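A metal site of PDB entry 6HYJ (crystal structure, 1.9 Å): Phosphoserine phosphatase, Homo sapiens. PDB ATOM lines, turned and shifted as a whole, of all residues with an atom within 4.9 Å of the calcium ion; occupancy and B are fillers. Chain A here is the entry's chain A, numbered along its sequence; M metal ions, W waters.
Water W2 lies within hydrogen-bond range of the side-chain carboxylate (OD2) of Asp 183 (2.5 Å), the side-chain amino group (NZ) of Lys 158 (3.3 Å) and the side-chain carboxylate (OD1) of Asp 20 (3.5 Å). Water W1 bridges OE2 of Glu 29 and OD2 of Asp 179.
Three residues have an atom within 4 Å of the calcium ion: Asp 20, Asp 22 and Asp 179.
The calcium ion is bound by OD1 of Asp 179, water W3, OD2 of Asp 20, O of Asp 22, water W2 and water W1. The calcium ion has six donor atoms within binding distance. Slightly farther from the calcium ion lies the side-chain carboxylate (OD1) of Asp 20 (3.1 Å).
OG1 of Thr 24 sits close to OD2 of Asp 20 (2.9 Å). OD1 of Asp 20 is in salt-bridge range of NZ of Lys 158 (2.9 Å). The backbone NH of Asp 179 is in hydrogen-bond range of the side-chain carboxylate of Asp 183 (3.3 Å). N of Asp 179 lies within hydrogen-bond range of OG1 of Thr 24 (3.1 Å).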
ATOM      1  N   ASP A  20      29.983  22.077  32.172  1.00  0.00           N
ATOM      2  CA  ASP A  20      29.173  21.630  31.063  1.00  0.00           C
ATOM      3  C   ASP A  20      27.692  21.766  31.444  1.00  0.00           C
ATOM      4  O   ASP A  20      27.334  21.623  32.602  1.00  0.00           O
ATOM      5  CB  ASP A  20      29.552  20.176  30.734  1.00  0.00           C
ATOM      6  CG  ASP A  20      28.546  19.492  29.825  1.00  0.00           C
ATOM      7  OD1 ASP A  20      28.316  19.972  28.700  1.00  0.00           O
ATOM      8  OD2 ASP A  20      27.991  18.463  30.264  1.00  0.00           O
ATOM      9  N   ASP A  22      24.519  20.440  29.422  1.00  0.00           N
ATOM     10  CA  ASP A  22      23.660  19.278  29.178  1.00  0.00           C
ATOM     11  C   ASP A  22      24.121  18.085  29.997  1.00  0.00           C
ATOM     12  O   ASP A  22      25.253  17.624  29.851  1.00  0.00           O
ATOM     13  CB  ASP A  22      23.655  18.907  27.697  1.00  0.00           C
ATOM     14  CG  ASP A  22      22.993  19.963  26.825  1.00  0.00           C
ATOM     15  OD1 ASP A  22      22.174  20.763  27.338  1.00  0.00           O
ATOM     16  OD2 ASP A  22      23.289  20.011  25.623  1.00  0.00           O
ATOM     17  N   SER A  23      23.237  17.548  30.836  1.00  0.00           N
ATOM     18  CA  SER A  23      23.445  16.361  31.650  1.00  0.00           C
ATOM     19  C   SER A  23      24.346  16.615  32.845  1.00  0.00           C
ATOM     20  O   SER A  23      24.610  15.677  33.611  1.00  0.00           O
ATOM     21  CB  SER A  23      24.019  15.180  30.840  1.00  0.00           C
ATOM     22  OG  SER A  23      23.100  14.748  29.863  1.00  0.00           O
ATOM     23  N   THR A  24      24.822  17.845  33.049  1.00  0.00           N
ATOM     24  CA  THR A  24      25.641  18.201  34.202  1.00  0.00           C
ATOM     25  C   THR A  24      24.890  19.240  35.019  1.00  0.00           C
ATOM     26  O   THR A  24      24.294  18.892  36.041  1.00  0.00           O
ATOM     27  CB  THR A  24      27.027  18.696  33.762  1.00  0.00           C
ATOM     28  OG1 THR A  24      27.712  17.652  33.074  1.00  0.00           O
ATOM     29  CG2 THR A  24      27.854  19.067  34.943  1.00  0.00           C
ATOM     30  N   GLU A  29      19.250  17.324  27.789  1.00  0.00           N
ATOM     31  CA  GLU A  29      20.078  17.869  26.730  1.00  0.00           C
ATOM     32  C   GLU A  29      19.252  18.935  26.045  1.00  0.00           C
ATOM     33  O   GLU A  29      18.224  18.621  25.437  1.00  0.00           O
ATOM     34  CB  GLU A  29      20.508  16.793  25.724  1.00  0.00           C
ATOM     35  CG  GLU A  29      21.116  15.582  26.360  1.00  0.00           C
ATOM     36  CD  GLU A  29      22.610  15.545  26.148  1.00  0.00           C
ATOM     37  OE1 GLU A  29      23.038  15.822  25.005  1.00  0.00           O
ATOM     38  OE2 GLU A  29      23.348  15.287  27.123  1.00  0.00           O
ATOM     39  N   LYS A 158      34.976  23.419  23.885  1.00  0.00           N
ATOM     40  CA  LYS A 158      35.125  23.646  25.314  1.00  0.00           C
ATOM     41  C   LYS A 158      36.560  24.013  25.674  1.00  0.00           C
ATOM     42  O   LYS A 158      36.787  24.964  26.427  1.00  0.00           O
ATOM     43  CB  LYS A 158      34.648  22.427  26.088  1.00  0.00           C
ATOM     44  CG  LYS A 158      33.134  22.378  26.132  1.00  0.00           C
ATOM     45  CD  LYS A 158      32.582  21.065  26.669  1.00  0.00           C
ATOM     46  CE  LYS A 158      31.058  21.063  26.537  1.00  0.00           C
ATOM     47  NZ  LYS A 158      30.491  19.707  26.800  1.00  0.00           N
ATOM     48  N   ASP A 179      29.986  15.778  32.218  1.00  0.00           N
ATOM     49  CA  ASP A 179      29.674  14.360  32.200  1.00  0.00           C
ATOM     50  C   ASP A 179      30.414  13.564  31.125  1.00  0.00           C
ATOM     51  O   ASP A 179      30.538  12.348  31.260  1.00  0.00           O
ATOM     52  CB  ASP A 179      28.174  14.175  31.995  1.00  0.00           C
ATOM     53  CG  ASP A 179      27.720  14.684  30.650  1.00  0.00           C
ATOM     54  OD1 ASP A 179      27.962  15.876  30.329  1.00  0.00           O
ATOM     55  OD2 ASP A 179      27.132  13.884  29.901  1.00  0.00           O
ATOM     56  N   ASP A 183      34.148  16.985  27.756  1.00  0.00           N
ATOM     57  CA  ASP A 183      34.523  17.750  28.930  1.00  0.00           C
ATOM     58  C   ASP A 183      35.855  17.269  29.472  1.00  0.00           C
ATOM     59  O   ASP A 183      36.729  18.064  29.829  1.00  0.00           O
ATOM     60  CB  ASP A 183      33.447  17.646  30.001  1.00  0.00           C
ATOM     61  CG  ASP A 183      32.081  17.945  29.449  1.00  0.00           C
ATOM     62  OD1 ASP A 183      31.878  19.094  28.994  1.00  0.00           O
ATOM     63  OD2 ASP A 183      31.233  17.033  29.413  1.00  0.00           O
HETATM   64 CA    CA M   1      27.169  17.078  28.690  1.00  0.00          CA
HETATM   65  O   HOH W   1      25.794  15.349  27.689  1.00  0.00           O
HETATM   66  O   HOH W   2      29.377  16.789  27.737  1.00  0.00           O
HETATM   67  O   HOH W   3      26.727  17.848  26.635  1.00  0.00           O
